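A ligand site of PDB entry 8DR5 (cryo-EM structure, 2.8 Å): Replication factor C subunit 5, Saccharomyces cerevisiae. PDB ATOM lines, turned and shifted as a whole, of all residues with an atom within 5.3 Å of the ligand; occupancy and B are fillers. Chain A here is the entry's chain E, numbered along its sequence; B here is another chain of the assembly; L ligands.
O of Ser 695 of chain B lies close to O6 of the ligand, 3.1 Å away.
OG of Ser 695 of chain B is in hydrogen-bond range of O6 of the ligand, at 2.6 Å.
O1 of the ligand sits at hydrogen-bond distance from N of Lys 49 (2.7 Å).
An oxygen (O1) of the ligand is in salt-bridge range of the side-chain amino group (NZ) of Lys 49.
N of Gly 46 sits at hydrogen-bond distance from O3 of the ligand (2.9 Å).
The backbone carbonyl oxygen (O) of Val 5 sits at hydrogen-bond distance from an oxygen (O10) of the ligand (2.9 Å).
NH1 of Arg 9 is in hydrogen-bond range of O9 of the ligand, 3.0 Å away.
N of Gly 48 is in hydrogen-bond range of O1 of the ligand.
The guanidinium group (NH2) of Arg 52 lies within hydrogen-bond range of an oxygen (O11) of the ligand, 3.1 Å away.
N of Ser 17 sits at hydrogen-bond distance from O11 of the ligand, 3.2 Å away.
N3 of the ligand lies within hydrogen-bond range of OG of Ser 17 (3.1 Å).
O5 of the ligand is in hydrogen-bond range of N of Thr 51 (3.2 Å).
An oxygen (O5) of the ligand is in hydrogen-bond range of the side-chain hydroxyl (OG1) of Thr 51, at 3.2 Å.
The backbone NH (N) of Lys 50 lies within hydrogen-bond range of an oxygen (O5) of the ligand (3.2 Å).
A ring nitrogen (NE2) of His 18 is in hydrogen-bond range of a nitrogen (N2) of the ligand (3.4 Å).
O6 of the ligand lies within salt-bridge range of NH1 of Arg 231, 3.3 Å away.
O of Ser 695 of chain B sits at hydrogen-bond distance from NH1 of Arg 231, 3.2 Å away.
The side-chain amino group (NZ) of Lys 49 sits at hydrogen-bond distance from the backbone carbonyl oxygen (O) of Pro 44, at 2.9 Å.
The side-chain amino group (NZ) of Lys 49 lies within salt-bridge range of the side-chain carboxylate (OD1) of Asp 172.
The backbone carbonyl oxygen (O) of Gly 46 sits at hydrogen-bond distance from the backbone NH (N) of Leu 230, 3.2 Å away.
The backbone carbonyl oxygen of Val 5 is in hydrogen-bond range of the guanidinium group of Arg 9 (3.5 Å).
NH1 of Arg 9 is in salt-bridge range of OD1 of Asp 6.
O of Gly 48 is in hydrogen-bond range of NH1 of Arg 52 (3.1 Å).
A ring nitrogen (NE2) of His 18 lies within hydrogen-bond range of the backbone carbonyl oxygen (O) of Thr 47, at 3.2 Å.
Pro 10 touches the ligand (CD to N5, 3.7 Å).
Leu 16 touches the ligand (CA to O11, 3.6 Å).
Asn 45 touches the ligand.
N of Thr 47 touches O1 of the ligand (3.7 Å).
CG2 of Ile 201 touches N4 of the ligand (3.7 Å).
Leu 230 touches the ligand.
Hydrophobic or aromatic side chains that line the ligand: Val 5, Pro 10, Leu 16, His 18, Ile 201 and Leu 230.
Of the 26 residues printed, 18 come within 4 Å of the ligand.
Along chain A the residues within 4 Å of the ligand span positions 5 to 231.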
ATOM      1  N   VAL A   5     -23.681  12.032 -19.455  1.00  0.00           N
ATOM      2  CA  VAL A   5     -23.388  10.655 -19.081  1.00  0.00           C
ATOM      3  C   VAL A   5     -24.614  10.001 -18.457  1.00  0.00           C
ATOM      4  O   VAL A   5     -24.879   8.810 -18.669  1.00  0.00           O
ATOM      5  CB  VAL A   5     -22.169  10.601 -18.140  1.00  0.00           C
ATOM      6  CG1 VAL A   5     -22.448  11.361 -16.856  1.00  0.00           C
ATOM      7  CG2 VAL A   5     -21.779   9.162 -17.848  1.00  0.00           C
ATOM      8  N   ASP A   6     -25.378  10.759 -17.667  1.00  0.00           N
ATOM      9  CA  ASP A   6     -26.556  10.233 -16.995  1.00  0.00           C
ATOM     10  C   ASP A   6     -27.861  10.499 -17.737  1.00  0.00           C
ATOM     11  O   ASP A   6     -28.833   9.779 -17.532  1.00  0.00           O
ATOM     12  CB  ASP A   6     -26.673  10.810 -15.585  1.00  0.00           C
ATOM     13  CG  ASP A   6     -25.370  10.729 -14.811  1.00  0.00           C
ATOM     14  OD1 ASP A   6     -24.843   9.607 -14.656  1.00  0.00           O
ATOM     15  OD2 ASP A   6     -24.883  11.781 -14.355  1.00  0.00           O
ATOM     16  N   TYR A   8     -28.537  10.201 -20.934  1.00  0.00           N
ATOM     17  CA  TYR A   8     -28.784   9.305 -22.062  1.00  0.00           C
ATOM     18  C   TYR A   8     -28.511   7.841 -21.700  1.00  0.00           C
ATOM     19  O   TYR A   8     -28.353   7.011 -22.604  1.00  0.00           O
ATOM     20  CB  TYR A   8     -27.942   9.720 -23.267  1.00  0.00           C
ATOM     21  CG  TYR A   8     -28.173  11.144 -23.692  1.00  0.00           C
ATOM     22  CD1 TYR A   8     -29.393  11.540 -24.209  1.00  0.00           C
ATOM     23  CD2 TYR A   8     -27.170  12.095 -23.576  1.00  0.00           C
ATOM     24  CE1 TYR A   8     -29.618  12.847 -24.595  1.00  0.00           C
ATOM     25  CE2 TYR A   8     -27.385  13.405 -23.964  1.00  0.00           C
ATOM     26  CZ  TYR A   8     -28.606  13.771 -24.471  1.00  0.00           C
ATOM     27  OH  TYR A   8     -28.822  15.077 -24.868  1.00  0.00           O
ATOM     28  N   ARG A   9     -28.447   7.523 -20.422  1.00  0.00           N
ATOM     29  CA  ARG A   9     -28.222   6.145 -20.022  1.00  0.00           C
ATOM     30  C   ARG A   9     -29.431   5.290 -20.421  1.00  0.00           C
ATOM     31  O   ARG A   9     -30.569   5.666 -20.122  1.00  0.00           O
ATOM     32  CB  ARG A   9     -27.992   6.048 -18.523  1.00  0.00           C
ATOM     33  CG  ARG A   9     -28.099   4.638 -17.962  1.00  0.00           C
ATOM     34  CD  ARG A   9     -27.315   4.496 -16.666  1.00  0.00           C
ATOM     35  NE  ARG A   9     -27.766   5.434 -15.652  1.00  0.00           N
ATOM     36  CZ  ARG A   9     -27.159   6.576 -15.341  1.00  0.00           C
ATOM     37  NH1 ARG A   9     -26.045   6.949 -15.946  1.00  0.00           N
ATOM     38  NH2 ARG A   9     -27.682   7.350 -14.393  1.00  0.00           N
ATOM     39  N   PRO A  10     -29.233   4.159 -21.109  1.00  0.00           N
ATOM     40  CA  PRO A  10     -30.376   3.314 -21.474  1.00  0.00           C
ATOM     41  C   PRO A  10     -31.071   2.756 -20.242  1.00  0.00           C
ATOM     42  O   PRO A  10     -30.450   2.526 -19.200  1.00  0.00           O
ATOM     43  CB  PRO A  10     -29.747   2.202 -22.314  1.00  0.00           C
ATOM     44  CG  PRO A  10     -28.317   2.173 -21.915  1.00  0.00           C
ATOM     45  CD  PRO A  10     -27.954   3.588 -21.574  1.00  0.00           C
ATOM     46  N   ALA A  15     -32.476  -1.064 -25.155  1.00  0.00           N
ATOM     47  CA  ALA A  15     -31.747   0.181 -25.364  1.00  0.00           C
ATOM     48  C   ALA A  15     -30.242   0.006 -25.323  1.00  0.00           C
ATOM     49  O   ALA A  15     -29.519   0.958 -25.653  1.00  0.00           O
ATOM     50  CB  ALA A  15     -32.176   1.215 -24.310  1.00  0.00           C
ATOM     51  N   LEU A  16     -29.740  -1.157 -24.930  1.00  0.00           N
ATOM     52  CA  LEU A  16     -28.307  -1.402 -24.935  1.00  0.00           C
ATOM     53  C   LEU A  16     -27.764  -1.336 -26.359  1.00  0.00           C
ATOM     54  O   LEU A  16     -28.427  -1.739 -27.320  1.00  0.00           O
ATOM     55  CB  LEU A  16     -27.990  -2.759 -24.315  1.00  0.00           C
ATOM     56  CG  LEU A  16     -28.595  -3.010 -22.929  1.00  0.00           C
ATOM     57  CD1 LEU A  16     -28.078  -4.315 -22.341  1.00  0.00           C
ATOM     58  CD2 LEU A  16     -28.291  -1.850 -21.989  1.00  0.00           C
ATOM     59  N   SER A  17     -26.542  -0.812 -26.494  1.00  0.00           N
ATOM     60  CA  SER A  17     -25.964  -0.534 -27.803  1.00  0.00           C
ATOM     61  C   SER A  17     -24.533  -1.050 -27.937  1.00  0.00           C
ATOM     62  O   SER A  17     -23.772  -0.541 -28.766  1.00  0.00           O
ATOM     63  CB  SER A  17     -26.007   0.965 -28.108  1.00  0.00           C
ATOM     64  OG  SER A  17     -24.931   1.635 -27.468  1.00  0.00           O
ATOM     65  N   HIS A  18     -24.127  -2.036 -27.133  1.00  0.00           N
ATOM     66  CA  HIS A  18     -22.825  -2.656 -27.329  1.00  0.00           C
ATOM     67  C   HIS A  18     -22.821  -4.011 -26.636  1.00  0.00           C
ATOM     68  O   HIS A  18     -23.530  -4.224 -25.647  1.00  0.00           O
ATOM     69  CB  HIS A  18     -21.691  -1.768 -26.819  1.00  0.00           C
ATOM     70  CG  HIS A  18     -21.672  -1.583 -25.328  1.00  0.00           C
ATOM     71  ND1 HIS A  18     -21.046  -2.464 -24.478  1.00  0.00           N
ATOM     72  CD2 HIS A  18     -22.200  -0.611 -24.542  1.00  0.00           C
ATOM     73  CE1 HIS A  18     -21.190  -2.047 -23.234  1.00  0.00           C
ATOM     74  NE2 HIS A  18     -21.884  -0.922 -23.252  1.00  0.00           N
ATOM     75  N   PRO A  44     -14.414  -4.755 -16.640  1.00  0.00           N
ATOM     76  CA  PRO A  44     -13.719  -3.480 -16.412  1.00  0.00           C
ATOM     77  C   PRO A  44     -14.682  -2.393 -15.943  1.00  0.00           C
ATOM     78  O   PRO A  44     -15.902  -2.492 -16.090  1.00  0.00           O
ATOM     79  CB  PRO A  44     -13.134  -3.146 -17.793  1.00  0.00           C
ATOM     80  CG  PRO A  44     -13.077  -4.444 -18.520  1.00  0.00           C
ATOM     81  CD  PRO A  44     -14.243  -5.236 -18.012  1.00  0.00           C
ATOM     82  N   ASN A  45     -14.100  -1.349 -15.364  1.00  0.00           N
ATOM     83  CA  ASN A  45     -14.892  -0.246 -14.837  1.00  0.00           C
ATOM     84  C   ASN A  45     -15.434   0.624 -15.974  1.00  0.00           C
ATOM     85  O   ASN A  45     -14.779   0.821 -16.996  1.00  0.00           O
ATOM     86  CB  ASN A  45     -14.051   0.622 -13.899  1.00  0.00           C
ATOM     87  CG  ASN A  45     -13.544  -0.151 -12.697  1.00  0.00           C
ATOM     88  OD1 ASN A  45     -13.379  -1.378 -12.757  1.00  0.00           O
ATOM     89  ND2 ASN A  45     -13.285   0.550 -11.609  1.00  0.00           N
ATOM     90  N   GLY A  46     -16.636   1.149 -15.763  1.00  0.00           N
ATOM     91  CA  GLY A  46     -17.241   2.045 -16.725  1.00  0.00           C
ATOM     92  C   GLY A  46     -17.780   1.390 -17.979  1.00  0.00           C
ATOM     93  O   GLY A  46     -18.152   2.093 -18.912  1.00  0.00           O
ATOM     94  N   THR A  47     -17.831   0.051 -18.007  1.00  0.00           N
ATOM     95  CA  THR A  47     -18.308  -0.641 -19.200  1.00  0.00           C
ATOM     96  C   THR A  47     -19.822  -0.604 -19.320  1.00  0.00           C
ATOM     97  O   THR A  47     -20.354  -0.601 -20.439  1.00  0.00           O
ATOM     98  CB  THR A  47     -17.815  -2.086 -19.198  1.00  0.00           C
ATOM     99  OG1 THR A  47     -18.301  -2.764 -18.034  1.00  0.00           O
ATOM    100  CG2 THR A  47     -16.299  -2.129 -19.202  1.00  0.00           C
ATOM    101  N   GLY A  48     -20.540  -0.581 -18.200  1.00  0.00           N
ATOM    102  CA  GLY A  48     -21.991  -0.602 -18.220  1.00  0.00           C
ATOM    103  C   GLY A  48     -22.592  -1.758 -17.447  1.00  0.00           C
ATOM    104  O   GLY A  48     -23.693  -2.211 -17.758  1.00  0.00           O
ATOM    105  N   LYS A  49     -21.877  -2.241 -16.433  1.00  0.00           N
ATOM    106  CA  LYS A  49     -22.356  -3.379 -15.653  1.00  0.00           C
ATOM    107  C   LYS A  49     -23.610  -3.026 -14.862  1.00  0.00           C
ATOM    108  O   LYS A  49     -24.597  -3.773 -14.868  1.00  0.00           O
ATOM    109  CB  LYS A  49     -21.253  -3.878 -14.723  1.00  0.00           C
ATOM    110  CG  LYS A  49     -20.008  -4.353 -15.441  1.00  0.00           C
ATOM    111  CD  LYS A  49     -19.084  -5.127 -14.511  1.00  0.00           C
ATOM    112  CE  LYS A  49     -18.535  -4.241 -13.400  1.00  0.00           C
ATOM    113  NZ  LYS A  49     -17.819  -3.057 -13.925  1.00  0.00           N
ATOM    114  N   LYS A  50     -23.588  -1.887 -14.160  1.00  0.00           N
ATOM    115  CA  LYS A  50     -24.755  -1.481 -13.393  1.00  0.00           C
ATOM    116  C   LYS A  50     -25.947  -1.188 -14.299  1.00  0.00           C
ATOM    117  O   LYS A  50     -27.096  -1.499 -13.946  1.00  0.00           O
ATOM    118  CB  LYS A  50     -24.423  -0.269 -12.525  1.00  0.00           C
ATOM    119  CG  LYS A  50     -24.119  -0.597 -11.069  1.00  0.00           C
ATOM    120  CD  LYS A  50     -25.338  -1.125 -10.330  1.00  0.00           C
ATOM    121  CE  LYS A  50     -26.037  -0.020  -9.546  1.00  0.00           C
ATOM    122  NZ  LYS A  50     -27.420  -0.412  -9.149  1.00  0.00           N
ATOM    123  N   THR A  51     -25.690  -0.591 -15.462  1.00  0.00           N
ATOM    124  CA  THR A  51     -26.767  -0.366 -16.417  1.00  0.00           C
ATOM    125  C   THR A  51     -27.392  -1.674 -16.851  1.00  0.00           C
ATOM    126  O   THR A  51     -28.620  -1.789 -16.939  1.00  0.00           O
ATOM    127  CB  THR A  51     -26.227   0.402 -17.625  1.00  0.00           C
ATOM    128  OG1 THR A  51     -25.635   1.629 -17.204  1.00  0.00           O
ATOM    129  CG2 THR A  51     -27.338   0.691 -18.621  1.00  0.00           C
ATOM    130  N   ARG A  52     -26.570  -2.694 -17.111  1.00  0.00           N
ATOM    131  CA  ARG A  52     -27.099  -3.993 -17.511  1.00  0.00           C
ATOM    132  C   ARG A  52     -27.867  -4.649 -16.379  1.00  0.00           C
ATOM    133  O   ARG A  52     -28.884  -5.304 -16.616  1.00  0.00           O
ATOM    134  CB  ARG A  52     -25.958  -4.887 -17.995  1.00  0.00           C
ATOM    135  CG  ARG A  52     -25.795  -4.900 -19.505  1.00  0.00           C
ATOM    136  CD  ARG A  52     -24.342  -4.881 -19.939  1.00  0.00           C
ATOM    137  NE  ARG A  52     -24.200  -4.359 -21.290  1.00  0.00           N
ATOM    138  CZ  ARG A  52     -24.377  -3.090 -21.635  1.00  0.00           C
ATOM    139  NH1 ARG A  52     -24.695  -2.167 -20.731  1.00  0.00           N
ATOM    140  NH2 ARG A  52     -24.243  -2.731 -22.909  1.00  0.00           N
ATOM    141  N   ASP A 172     -15.554  -5.414 -10.030  1.00  0.00           N
ATOM    142  CA  ASP A 172     -14.594  -5.122 -11.084  1.00  0.00           C
ATOM    143  C   ASP A 172     -13.555  -6.225 -11.236  1.00  0.00           C
ATOM    144  O   ASP A 172     -13.099  -6.483 -12.354  1.00  0.00           O
ATOM    145  CB  ASP A 172     -13.896  -3.788 -10.813  1.00  0.00           C
ATOM    146  CG  ASP A 172     -14.881  -2.667 -10.555  1.00  0.00           C
ATOM    147  OD1 ASP A 172     -15.494  -2.178 -11.515  1.00  0.00           O
ATOM    148  OD2 ASP A 172     -15.022  -2.260  -9.381  1.00  0.00           O
ATOM    149  N   ILE A 201     -21.766   5.917 -29.806  1.00  0.00           N
ATOM    150  CA  ILE A 201     -22.491   6.487 -28.680  1.00  0.00           C
ATOM    151  C   ILE A 201     -22.192   7.979 -28.552  1.00  0.00           C
ATOM    152  O   ILE A 201     -23.103   8.791 -28.342  1.00  0.00           O
ATOM    153  CB  ILE A 201     -22.131   5.733 -27.380  1.00  0.00           C
ATOM    154  CG1 ILE A 201     -22.708   4.311 -27.429  1.00  0.00           C
ATOM    155  CG2 ILE A 201     -22.668   6.477 -26.167  1.00  0.00           C
ATOM    156  CD1 ILE A 201     -22.063   3.360 -26.441  1.00  0.00           C
ATOM    157  N   LEU A 230     -16.441   3.887 -20.867  1.00  0.00           N
ATOM    158  CA  LEU A 230     -17.482   4.683 -21.510  1.00  0.00           C
ATOM    159  C   LEU A 230     -17.859   5.902 -20.681  1.00  0.00           C
ATOM    160  O   LEU A 230     -18.094   6.988 -21.235  1.00  0.00           O
ATOM    161  CB  LEU A 230     -18.707   3.811 -21.775  1.00  0.00           C
ATOM    162  CG  LEU A 230     -19.853   4.420 -22.592  1.00  0.00           C
ATOM    163  CD1 LEU A 230     -19.340   5.095 -23.862  1.00  0.00           C
ATOM    164  CD2 LEU A 230     -20.880   3.347 -22.929  1.00  0.00           C
ATOM    165  N   ARG A 231     -17.923   5.746 -19.354  1.00  0.00           N
ATOM    166  CA  ARG A 231     -18.232   6.888 -18.493  1.00  0.00           C
ATOM    167  C   ARG A 231     -17.182   7.975 -18.649  1.00  0.00           C
ATOM    168  O   ARG A 231     -17.513   9.170 -18.767  1.00  0.00           O
ATOM    169  CB  ARG A 231     -18.321   6.425 -17.038  1.00  0.00           C
ATOM    170  CG  ARG A 231     -18.224   7.547 -16.018  1.00  0.00           C
ATOM    171  CD  ARG A 231     -18.592   7.079 -14.617  1.00  0.00           C
ATOM    172  NE  ARG A 231     -17.716   6.016 -14.136  1.00  0.00           N
ATOM    173  CZ  ARG A 231     -18.097   4.777 -13.837  1.00  0.00           C
ATOM    174  NH1 ARG A 231     -19.354   4.391 -13.959  1.00  0.00           N
ATOM    175  NH2 ARG A 231     -17.186   3.902 -13.422  1.00  0.00           N
ATOM    176  N   LEU A 234     -17.713   9.783 -22.010  1.00  0.00           N
ATOM    177  CA  LEU A 234     -18.805  10.756 -22.012  1.00  0.00           C
ATOM    178  C   LEU A 234     -18.430  12.000 -21.222  1.00  0.00           C
ATOM    179  O   LEU A 234     -18.671  13.128 -21.673  1.00  0.00           O
ATOM    180  CB  LEU A 234     -20.074  10.112 -21.452  1.00  0.00           C
ATOM    181  CG  LEU A 234     -20.772   9.134 -22.395  1.00  0.00           C
ATOM    182  CD1 LEU A 234     -21.529   8.064 -21.609  1.00  0.00           C
ATOM    183  CD2 LEU A 234     -21.717   9.869 -23.321  1.00  0.00           C
ATOM    184  N   SER B 695     -24.615   7.190 -11.914  1.00  0.00           N
ATOM    185  CA  SER B 695     -24.380   5.757 -12.004  1.00  0.00           C
ATOM    186  C   SER B 695     -22.882   5.517 -11.782  1.00  0.00           C
ATOM    187  O   SER B 695     -22.104   5.443 -12.741  1.00  0.00           O
ATOM    188  CB  SER B 695     -24.833   5.198 -13.349  1.00  0.00           C
ATOM    189  OG  SER B 695     -24.523   3.821 -13.474  1.00  0.00           O
ATOM    190  N   THR B 696     -22.484   5.397 -10.519  1.00  0.00           N
ATOM    191  CA  THR B 696     -21.091   5.199 -10.167  1.00  0.00           C
ATOM    192  C   THR B 696     -20.943   4.980  -8.663  1.00  0.00           C
ATOM    193  O   THR B 696     -21.916   5.110  -7.920  1.00  0.00           O
ATOM    194  CB  THR B 696     -20.238   6.384 -10.617  1.00  0.00           C
ATOM    195  OG1 THR B 696     -18.859   6.156 -10.274  1.00  0.00           O
ATOM    196  CG2 THR B 696     -20.711   7.677  -9.944  1.00  0.00           C
ATOM    197  N   TYR B 705     -16.367  12.004 -12.157  1.00  0.00           N
ATOM    198  CA  TYR B 705     -17.485  12.932 -12.205  1.00  0.00           C
ATOM    199  C   TYR B 705     -17.083  14.336 -11.767  1.00  0.00           C
ATOM    200  O   TYR B 705     -17.442  15.320 -12.416  1.00  0.00           O
ATOM    201  CB  TYR B 705     -18.634  12.413 -11.336  1.00  0.00           C
ATOM    202  CG  TYR B 705     -19.653  11.586 -12.075  1.00  0.00           C
ATOM    203  CD1 TYR B 705     -20.769  12.178 -12.666  1.00  0.00           C
ATOM    204  CD2 TYR B 705     -19.511  10.214 -12.190  1.00  0.00           C
ATOM    205  CE1 TYR B 705     -21.704  11.430 -13.342  1.00  0.00           C
ATOM    206  CE2 TYR B 705     -20.441   9.448 -12.861  1.00  0.00           C
ATOM    207  CZ  TYR B 705     -21.539  10.061 -13.439  1.00  0.00           C
ATOM    208  OH  TYR B 705     -22.462   9.306 -14.114  1.00  0.00           O
HETATM  209  P1  LIG L   1     -19.959   0.308 -14.361  1.00  0.00           P
HETATM  210  O1  LIG L   1     -19.871  -1.021 -15.080  1.00  0.00           O
HETATM  211  O2  LIG L   1     -20.999   0.223 -13.266  1.00  0.00           O
HETATM  212  O3  LIG L   1     -18.615   0.644 -13.763  1.00  0.00           O
HETATM  213  O4  LIG L   1     -20.385   1.485 -15.441  1.00  0.00           O
HETATM  214  P2  LIG L   1     -21.922   2.028 -15.668  1.00  0.00           P
HETATM  215  O5  LIG L   1     -22.883   0.862 -15.672  1.00  0.00           O
HETATM  216  O6  LIG L   1     -22.295   2.967 -14.554  1.00  0.00           O
HETATM  217  O7  LIG L   1     -21.999   2.816 -17.105  1.00  0.00           O
HETATM  218  C1  LIG L   1     -21.302   4.031 -17.238  1.00  0.00           C
HETATM  219  C2  LIG L   1     -22.001   4.940 -18.239  1.00  0.00           C
HETATM  220  O8  LIG L   1     -21.901   4.275 -19.703  1.00  0.00           O
HETATM  221  C3  LIG L   1     -23.268   5.089 -17.939  1.00  0.00           C
HETATM  222  O9  LIG L   1     -23.490   6.460 -17.405  1.00  0.00           O
HETATM  223  C4  LIG L   1     -24.055   4.908 -19.252  1.00  0.00           C
HETATM  224  O10 LIG L   1     -24.574   6.103 -19.633  1.00  0.00           O
HETATM  225  C5  LIG L   1     -23.056   4.413 -20.306  1.00  0.00           C
HETATM  226  N1  LIG L   1     -23.465   3.098 -20.837  1.00  0.00           N
HETATM  227  C6  LIG L   1     -23.305   1.879 -20.317  1.00  0.00           C
HETATM  228  N2  LIG L   1     -23.848   0.995 -21.186  1.00  0.00           N
HETATM  229  C7  LIG L   1     -24.338   1.684 -22.223  1.00  0.00           C
HETATM  230  C8  LIG L   1     -25.057   1.231 -23.491  1.00  0.00           C
HETATM  231  O11 LIG L   1     -25.268   0.087 -23.680  1.00  0.00           O
HETATM  232  N3  LIG L   1     -25.474   2.205 -24.460  1.00  0.00           N
HETATM  233  C9  LIG L   1     -25.216   3.599 -24.221  1.00  0.00           C
HETATM  234  N4  LIG L   1     -25.639   4.591 -25.195  1.00  0.00           N
HETATM  235  N5  LIG L   1     -24.529   4.025 -23.005  1.00  0.00           N
HETATM  236  C10 LIG L   1     -24.097   3.009 -22.012  1.00  0.00           C
